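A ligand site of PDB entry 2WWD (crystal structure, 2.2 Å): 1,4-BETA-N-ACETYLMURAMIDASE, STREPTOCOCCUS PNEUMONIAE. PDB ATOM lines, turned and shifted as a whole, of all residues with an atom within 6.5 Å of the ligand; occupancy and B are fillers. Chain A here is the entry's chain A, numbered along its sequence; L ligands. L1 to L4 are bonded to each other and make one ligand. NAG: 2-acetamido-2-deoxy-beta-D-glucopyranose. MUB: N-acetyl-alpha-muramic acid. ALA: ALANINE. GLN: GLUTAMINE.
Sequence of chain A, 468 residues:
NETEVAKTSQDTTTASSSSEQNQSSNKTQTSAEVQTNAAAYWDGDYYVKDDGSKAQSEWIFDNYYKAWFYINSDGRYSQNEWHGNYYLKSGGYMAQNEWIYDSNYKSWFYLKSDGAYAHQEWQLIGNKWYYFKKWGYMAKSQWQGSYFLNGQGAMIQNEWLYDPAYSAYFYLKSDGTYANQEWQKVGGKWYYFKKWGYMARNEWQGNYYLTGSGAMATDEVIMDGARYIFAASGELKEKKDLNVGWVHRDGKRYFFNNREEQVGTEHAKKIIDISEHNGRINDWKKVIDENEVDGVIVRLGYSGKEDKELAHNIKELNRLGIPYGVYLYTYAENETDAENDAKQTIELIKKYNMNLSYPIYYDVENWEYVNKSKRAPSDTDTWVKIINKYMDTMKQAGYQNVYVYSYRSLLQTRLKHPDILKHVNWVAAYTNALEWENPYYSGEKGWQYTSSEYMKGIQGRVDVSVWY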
ATOM      1  N   ASP A 219     -13.602 -20.185  17.029  1.00  0.00           N
ATOM      2  CA  ASP A 219     -14.930 -19.559  17.027  1.00  0.00           C
ATOM      3  C   ASP A 219     -15.980 -20.265  16.162  1.00  0.00           C
ATOM      4  O   ASP A 219     -16.770 -21.054  16.676  1.00  0.00           O
ATOM      5  CB  ASP A 219     -14.836 -18.052  16.711  1.00  0.00           C
ATOM      6  CG  ASP A 219     -13.877 -17.739  15.565  1.00  0.00           C
ATOM      7  OD1 ASP A 219     -13.949 -18.401  14.509  1.00  0.00           O
ATOM      8  OD2 ASP A 219     -13.051 -16.808  15.733  1.00  0.00           O
ATOM      9  N   TYR A 329      -2.700  -8.046 -13.913  1.00  0.00           N
ATOM     10  CA  TYR A 329      -2.072  -7.859 -12.610  1.00  0.00           C
ATOM     11  C   TYR A 329      -0.980  -6.791 -12.724  1.00  0.00           C
ATOM     12  O   TYR A 329      -0.057  -6.921 -13.512  1.00  0.00           O
ATOM     13  CB  TYR A 329      -1.471  -9.177 -12.105  1.00  0.00           C
ATOM     14  CG  TYR A 329      -0.930  -9.110 -10.691  1.00  0.00           C
ATOM     15  CD1 TYR A 329      -1.751  -9.401  -9.592  1.00  0.00           C
ATOM     16  CD2 TYR A 329       0.402  -8.742 -10.449  1.00  0.00           C
ATOM     17  CE1 TYR A 329      -1.245  -9.348  -8.295  1.00  0.00           C
ATOM     18  CE2 TYR A 329       0.912  -8.676  -9.157  1.00  0.00           C
ATOM     19  CZ  TYR A 329       0.083  -8.976  -8.084  1.00  0.00           C
ATOM     20  OH  TYR A 329       0.589  -8.910  -6.814  1.00  0.00           O
ATOM     21  N   ASP A 363      -6.064  -5.088 -11.991  1.00  0.00           N
ATOM     22  CA  ASP A 363      -5.888  -5.874 -10.770  1.00  0.00           C
ATOM     23  C   ASP A 363      -4.835  -5.213  -9.859  1.00  0.00           C
ATOM     24  O   ASP A 363      -3.627  -5.360 -10.075  1.00  0.00           O
ATOM     25  CB  ASP A 363      -5.490  -7.303 -11.173  1.00  0.00           C
ATOM     26  CG  ASP A 363      -5.304  -8.231  -9.986  1.00  0.00           C
ATOM     27  OD1 ASP A 363      -5.358  -7.776  -8.826  1.00  0.00           O
ATOM     28  OD2 ASP A 363      -5.102  -9.443 -10.220  1.00  0.00           O
ATOM     29  N   GLU A 365      -3.078  -4.835  -6.255  1.00  0.00           N
ATOM     30  CA  GLU A 365      -2.785  -5.541  -5.010  1.00  0.00           C
ATOM     31  C   GLU A 365      -1.488  -5.029  -4.381  1.00  0.00           C
ATOM     32  O   GLU A 365      -0.790  -4.195  -4.962  1.00  0.00           O
ATOM     33  CB  GLU A 365      -2.707  -7.048  -5.258  1.00  0.00           C
ATOM     34  CG  GLU A 365      -3.997  -7.637  -5.879  1.00  0.00           C
ATOM     35  CD  GLU A 365      -3.982  -9.148  -5.985  1.00  0.00           C
ATOM     36  OE1 GLU A 365      -4.579  -9.669  -6.947  1.00  0.00           O
ATOM     37  OE2 GLU A 365      -3.388  -9.819  -5.113  1.00  0.00           O
ATOM     38  N   ASN A 366      -1.158  -5.533  -3.197  1.00  0.00           N
ATOM     39  CA  ASN A 366       0.084  -5.180  -2.508  1.00  0.00           C
ATOM     40  C   ASN A 366       1.206  -6.027  -3.092  1.00  0.00           C
ATOM     41  O   ASN A 366       1.637  -7.015  -2.486  1.00  0.00           O
ATOM     42  CB  ASN A 366      -0.052  -5.393  -0.996  1.00  0.00           C
ATOM     43  CG  ASN A 366       1.151  -4.893  -0.205  1.00  0.00           C
ATOM     44  OD1 ASN A 366       1.689  -3.816  -0.451  1.00  0.00           O
ATOM     45  ND2 ASN A 366       1.561  -5.690   0.776  1.00  0.00           N
ATOM     46  N   TYR A 405      -9.974  -3.818  -9.842  1.00  0.00           N
ATOM     47  CA  TYR A 405     -10.229  -4.925  -8.941  1.00  0.00           C
ATOM     48  C   TYR A 405      -9.215  -4.870  -7.804  1.00  0.00           C
ATOM     49  O   TYR A 405      -8.026  -4.628  -8.026  1.00  0.00           O
ATOM     50  CB  TYR A 405     -10.147  -6.269  -9.676  1.00  0.00           C
ATOM     51  CG  TYR A 405      -9.819  -7.451  -8.784  1.00  0.00           C
ATOM     52  CD1 TYR A 405     -10.832  -8.322  -8.349  1.00  0.00           C
ATOM     53  CD2 TYR A 405      -8.505  -7.698  -8.364  1.00  0.00           C
ATOM     54  CE1 TYR A 405     -10.538  -9.407  -7.533  1.00  0.00           C
ATOM     55  CE2 TYR A 405      -8.207  -8.775  -7.545  1.00  0.00           C
ATOM     56  CZ  TYR A 405      -9.220  -9.633  -7.137  1.00  0.00           C
ATOM     57  OH  TYR A 405      -8.919 -10.697  -6.322  1.00  0.00           O
ATOM     58  N   SER A 406      -9.689  -5.112  -6.587  1.00  0.00           N
ATOM     59  CA  SER A 406      -8.796  -5.295  -5.437  1.00  0.00           C
ATOM     60  C   SER A 406      -9.529  -6.077  -4.347  1.00  0.00           C
ATOM     61  O   SER A 406     -10.686  -6.462  -4.533  1.00  0.00           O
ATOM     62  CB  SER A 406      -8.282  -3.947  -4.918  1.00  0.00           C
ATOM     63  OG  SER A 406      -7.188  -4.127  -4.034  1.00  0.00           O
ATOM     64  N   TYR A 407      -8.844  -6.321  -3.234  1.00  0.00           N
ATOM     65  CA  TYR A 407      -9.431  -6.967  -2.060  1.00  0.00           C
ATOM     66  C   TYR A 407      -9.771  -5.956  -0.980  1.00  0.00           C
ATOM     67  O   TYR A 407      -9.139  -4.899  -0.884  1.00  0.00           O
ATOM     68  CB  TYR A 407      -8.508  -8.058  -1.497  1.00  0.00           C
ATOM     69  CG  TYR A 407      -7.067  -7.629  -1.306  1.00  0.00           C
ATOM     70  CD1 TYR A 407      -6.639  -7.066  -0.102  1.00  0.00           C
ATOM     71  CD2 TYR A 407      -6.127  -7.812  -2.328  1.00  0.00           C
ATOM     72  CE1 TYR A 407      -5.315  -6.689   0.079  1.00  0.00           C
ATOM     73  CE2 TYR A 407      -4.812  -7.424  -2.165  1.00  0.00           C
ATOM     74  CZ  TYR A 407      -4.406  -6.862  -0.961  1.00  0.00           C
ATOM     75  OH  TYR A 407      -3.104  -6.484  -0.791  1.00  0.00           O
ATOM     76  N   ARG A 408     -10.779  -6.306  -0.171  1.00  0.00           N
ATOM     77  CA  ARG A 408     -11.442  -5.440   0.802  1.00  0.00           C
ATOM     78  C   ARG A 408     -10.514  -4.598   1.688  1.00  0.00           C
ATOM     79  O   ARG A 408     -10.653  -3.370   1.752  1.00  0.00           O
ATOM     80  CB  ARG A 408     -12.373  -6.284   1.667  1.00  0.00           C
ATOM     81  CG  ARG A 408     -13.243  -5.520   2.639  1.00  0.00           C
ATOM     82  CD  ARG A 408     -14.244  -6.474   3.245  1.00  0.00           C
ATOM     83  NE  ARG A 408     -14.849  -5.925   4.445  1.00  0.00           N
ATOM     84  CZ  ARG A 408     -14.682  -6.425   5.666  1.00  0.00           C
ATOM     85  NH1 ARG A 408     -13.927  -7.506   5.849  1.00  0.00           N
ATOM     86  NH2 ARG A 408     -15.281  -5.840   6.706  1.00  0.00           N
ATOM     87  N   SER A 409      -9.577  -5.262   2.360  1.00  0.00           N
ATOM     88  CA  SER A 409      -8.669  -4.600   3.295  1.00  0.00           C
ATOM     89  C   SER A 409      -7.896  -3.450   2.650  1.00  0.00           C
ATOM     90  O   SER A 409      -7.674  -2.419   3.280  1.00  0.00           O
ATOM     91  CB  SER A 409      -7.702  -5.601   3.932  1.00  0.00           C
ATOM     92  OG  SER A 409      -6.752  -6.046   2.986  1.00  0.00           O
ATOM     93  N   LEU A 410      -7.491  -3.644   1.398  1.00  0.00           N
ATOM     94  CA  LEU A 410      -6.753  -2.611   0.655  1.00  0.00           C
ATOM     95  C   LEU A 410      -7.639  -1.441   0.217  1.00  0.00           C
ATOM     96  O   LEU A 410      -7.191  -0.306   0.209  1.00  0.00           O
ATOM     97  CB  LEU A 410      -6.030  -3.215  -0.560  1.00  0.00           C
ATOM     98  CG  LEU A 410      -4.742  -2.530  -1.019  1.00  0.00           C
ATOM     99  CD1 LEU A 410      -3.672  -2.571   0.072  1.00  0.00           C
ATOM    100  CD2 LEU A 410      -4.225  -3.168  -2.303  1.00  0.00           C
ATOM    101  N   GLN A 412     -10.050  -0.458   1.938  1.00  0.00           N
ATOM    102  CA  GLN A 412     -10.333   0.178   3.218  1.00  0.00           C
ATOM    103  C   GLN A 412      -9.159   1.041   3.681  1.00  0.00           C
ATOM    104  O   GLN A 412      -9.351   1.976   4.459  1.00  0.00           O
ATOM    105  CB  GLN A 412     -10.626  -0.873   4.288  1.00  0.00           C
ATOM    106  CG  GLN A 412     -12.030  -1.476   4.214  1.00  0.00           C
ATOM    107  CD  GLN A 412     -12.220  -2.659   5.144  1.00  0.00           C
ATOM    108  OE1 GLN A 412     -13.339  -2.909   5.605  1.00  0.00           O
ATOM    109  NE2 GLN A 412     -11.147  -3.391   5.431  1.00  0.00           N
ATOM    110  N   ALA A 428     -12.682  -8.509  -3.948  1.00  0.00           N
ATOM    111  CA  ALA A 428     -12.406  -9.808  -3.319  1.00  0.00           C
ATOM    112  C   ALA A 428     -12.532  -9.708  -1.805  1.00  0.00           C
ATOM    113  O   ALA A 428     -12.013  -8.776  -1.180  1.00  0.00           O
ATOM    114  CB  ALA A 428     -11.011 -10.303  -3.687  1.00  0.00           C
ATOM    115  N   ALA A 429     -13.250 -10.667  -1.216  1.00  0.00           N
ATOM    116  CA  ALA A 429     -13.288 -10.846   0.235  1.00  0.00           C
ATOM    117  C   ALA A 429     -13.733 -12.279   0.479  1.00  0.00           C
ATOM    118  O   ALA A 429     -14.919 -12.609   0.330  1.00  0.00           O
ATOM    119  CB  ALA A 429     -14.251  -9.849   0.886  1.00  0.00           C
ATOM    120  N   TYR A 430     -12.780 -13.138   0.818  1.00  0.00           N
ATOM    121  CA  TYR A 430     -13.054 -14.554   1.025  1.00  0.00           C
ATOM    122  C   TYR A 430     -13.581 -14.738   2.445  1.00  0.00           C
ATOM    123  O   TYR A 430     -12.918 -15.329   3.309  1.00  0.00           O
ATOM    124  CB  TYR A 430     -11.824 -15.419   0.740  1.00  0.00           C
ATOM    125  CG  TYR A 430     -11.161 -15.128  -0.600  1.00  0.00           C
ATOM    126  CD1 TYR A 430     -11.892 -14.599  -1.679  1.00  0.00           C
ATOM    127  CD2 TYR A 430      -9.815 -15.414  -0.793  1.00  0.00           C
ATOM    128  CE1 TYR A 430     -11.268 -14.326  -2.894  1.00  0.00           C
ATOM    129  CE2 TYR A 430      -9.194 -15.149  -2.012  1.00  0.00           C
ATOM    130  CZ  TYR A 430      -9.927 -14.612  -3.054  1.00  0.00           C
ATOM    131  OH  TYR A 430      -9.297 -14.358  -4.257  1.00  0.00           O
ATOM    132  N   THR A 431     -14.790 -14.210   2.650  1.00  0.00           N
ATOM    133  CA  THR A 431     -15.393 -14.028   3.955  1.00  0.00           C
ATOM    134  C   THR A 431     -16.838 -14.516   3.923  1.00  0.00           C
ATOM    135  O   THR A 431     -17.321 -14.976   2.878  1.00  0.00           O
ATOM    136  CB  THR A 431     -15.372 -12.525   4.355  1.00  0.00           C
ATOM    137  OG1 THR A 431     -16.180 -11.767   3.437  1.00  0.00           O
ATOM    138  CG2 THR A 431     -13.946 -11.960   4.312  1.00  0.00           C
ATOM    139  N   GLN A 448     -15.860 -11.358  -5.439  1.00  0.00           N
ATOM    140  CA  GLN A 448     -15.059 -12.577  -5.463  1.00  0.00           C
ATOM    141  C   GLN A 448     -14.989 -13.113  -4.048  1.00  0.00           C
ATOM    142  O   GLN A 448     -14.247 -12.605  -3.215  1.00  0.00           O
ATOM    143  CB  GLN A 448     -13.675 -12.283  -6.028  1.00  0.00           C
ATOM    144  CG  GLN A 448     -12.867 -13.513  -6.366  1.00  0.00           C
ATOM    145  CD  GLN A 448     -11.444 -13.186  -6.706  1.00  0.00           C
ATOM    146  OE1 GLN A 448     -10.705 -12.649  -5.882  1.00  0.00           O
ATOM    147  NE2 GLN A 448     -11.042 -13.500  -7.927  1.00  0.00           N
HETATM  148  C1  NAG L   1      -4.719 -11.594  -0.904  1.00  0.00           C
HETATM  149  C2  NAG L   1      -3.782 -12.746  -1.274  1.00  0.00           C
HETATM  150  C3  NAG L   1      -3.350 -12.631  -2.736  1.00  0.00           C
HETATM  151  C4  NAG L   1      -4.583 -12.596  -3.641  1.00  0.00           C
HETATM  152  C5  NAG L   1      -5.590 -11.539  -3.182  1.00  0.00           C
HETATM  153  C6  NAG L   1      -6.904 -11.689  -3.941  1.00  0.00           C
HETATM  154  C7  NAG L   1      -2.267 -13.434   0.516  1.00  0.00           C
HETATM  155  C8  NAG L   1      -0.978 -13.150   1.238  1.00  0.00           C
HETATM  156  N2  NAG L   1      -2.559 -12.596  -0.481  1.00  0.00           N
HETATM  157  O3  NAG L   1      -2.500 -13.734  -3.082  1.00  0.00           O
HETATM  158  O4  NAG L   1      -4.175 -12.321  -4.996  1.00  0.00           O
HETATM  159  O5  NAG L   1      -5.861 -11.624  -1.774  1.00  0.00           O
HETATM  160  O6  NAG L   1      -7.539 -10.409  -4.001  1.00  0.00           O
HETATM  161  O7  NAG L   1      -3.007 -14.355   0.836  1.00  0.00           O
HETATM  162  C1  MUB L   2      -6.015  -9.039   3.606  1.00  0.00           C
HETATM  163  C2  MUB L   2      -7.120  -9.354   2.580  1.00  0.00           C
HETATM  164  C3  MUB L   2      -6.816 -10.590   1.738  1.00  0.00           C
HETATM  165  C4  MUB L   2      -5.422 -10.487   1.118  1.00  0.00           C
HETATM  166  C5  MUB L   2      -4.365 -10.144   2.179  1.00  0.00           C
HETATM  167  C6  MUB L   2      -3.002  -9.856   1.568  1.00  0.00           C
HETATM  168  C7  MUB L   2      -9.456  -8.886   3.069  1.00  0.00           C
HETATM  169  C8  MUB L   2     -10.700  -9.247   3.833  1.00  0.00           C
HETATM  170  C9  MUB L   2      -8.356 -11.994   0.456  1.00  0.00           C
HETATM  171  C10 MUB L   2      -9.154 -12.501   1.620  1.00  0.00           C
HETATM  172  C11 MUB L   2      -9.228 -11.858  -0.793  1.00  0.00           C
HETATM  173  O1  MUB L   2      -5.961 -10.003   4.657  1.00  0.00           O
HETATM  174  O3  MUB L   2      -7.826 -10.691   0.723  1.00  0.00           O
HETATM  175  O4  MUB L   2      -5.110 -11.728   0.461  1.00  0.00           O
HETATM  176  O5  MUB L   2      -4.759  -8.970   2.927  1.00  0.00           O
HETATM  177  O6  MUB L   2      -1.969 -10.039   2.539  1.00  0.00           O
HETATM  178  O7  MUB L   2      -9.450  -7.944   2.293  1.00  0.00           O
HETATM  179  O10 MUB L   2     -10.253 -12.053   1.874  1.00  0.00           O
HETATM  180  N2  MUB L   2      -8.379  -9.638   3.291  1.00  0.00           N
HETATM  181  N   ALA L   3      -8.576 -13.463   2.345  1.00  0.00           N
HETATM  182  CA  ALA L   3      -9.222 -14.058   3.511  1.00  0.00           C
HETATM  183  C   ALA L   3      -9.096 -13.168   4.738  1.00  0.00           C
HETATM  184  O   ALA L   3      -8.222 -12.316   4.781  1.00  0.00           O
HETATM  185  CB  ALA L   3      -8.595 -15.424   3.762  1.00  0.00           C
HETATM  186  N   GLN L   4      -9.977 -13.360   5.729  1.00  0.00           N
HETATM  187  CA  GLN L   4      -9.962 -12.583   6.972  1.00  0.00           C
HETATM  188  C   GLN L   4     -10.633 -11.236   6.877  1.00  0.00           C
HETATM  189  O   GLN L   4     -10.009 -10.207   7.171  1.00  0.00           O
HETATM  190  CB  GLN L   4     -10.697 -13.460   7.985  1.00  0.00           C
HETATM  191  CG  GLN L   4      -9.734 -14.267   8.844  1.00  0.00           C
HETATM  192  CD  GLN L   4     -10.286 -14.417  10.237  1.00  0.00           C
HETATM  193  OE1 GLN L   4     -11.218 -15.171  10.472  1.00  0.00           O
HETATM  194  OXT GLN L   4     -11.846 -11.214   6.495  1.00  0.00           O
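OE2 of Glu 365 sits at hydrogen-bond distance from O4 of NAG L1, at 2.6 Å. N of Ser 409 lies within hydrogen-bond range of O7 of MUB L2 (2.7 Å). O7 of MUB L2 sits close to OG of Ser 409, 3.4 Å away. An oxygen (O6) of NAG L1 is in hydrogen-bond range of the side-chain hydroxyl of Tyr 405 (2.7 Å). N of Tyr 430 lies within hydrogen-bond range of O10 of MUB L2 (2.9 Å). The backbone NH of Arg 408 is in hydrogen-bond range of an oxygen (O7) of MUB L2, 3.2 Å away.
The side-chain amide oxygen (OE1) of Gln 448 lies within hydrogen-bond range of the side-chain hydroxyl (OH) of Tyr 405 (2.7 Å). The side-chain amide oxygen (OE1) of Gln 448 is in hydrogen-bond range of the side-chain hydroxyl (OH) of Tyr 430, 2.7 Å away. The backbone carbonyl oxygen (O) of Ala 429 lies within hydrogen-bond range of the side-chain hydroxyl (OG1) of Thr 431 (3.5 Å). N of Arg 408 is in hydrogen-bond range of O of Ala 428, at 2.9 Å. OH of Tyr 407 is in hydrogen-bond range of N of Asn 366, 3.2 Å away. The backbone carbonyl oxygen (O) of Ser 406 is in hydrogen-bond range of the backbone NH (N) of Ala 428 (2.9 Å). The backbone NH (N) of Ala 429 lies within hydrogen-bond range of the backbone carbonyl oxygen (O) of Gln 448, 3.0 Å away.
Merely in contact with the ligand: Tyr 407, Ala 428, Ala 429 and Thr 431. Hydrophobic or aromatic side chains that line the ligand: Tyr 405, Tyr 407, Ala 428 and Tyr 430. Within 4 Å of the ligand: Glu 365, Tyr 405, Tyr 407, Arg 408, Ser 409, Ala 428, Ala 429, Tyr 430 and Thr 431.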
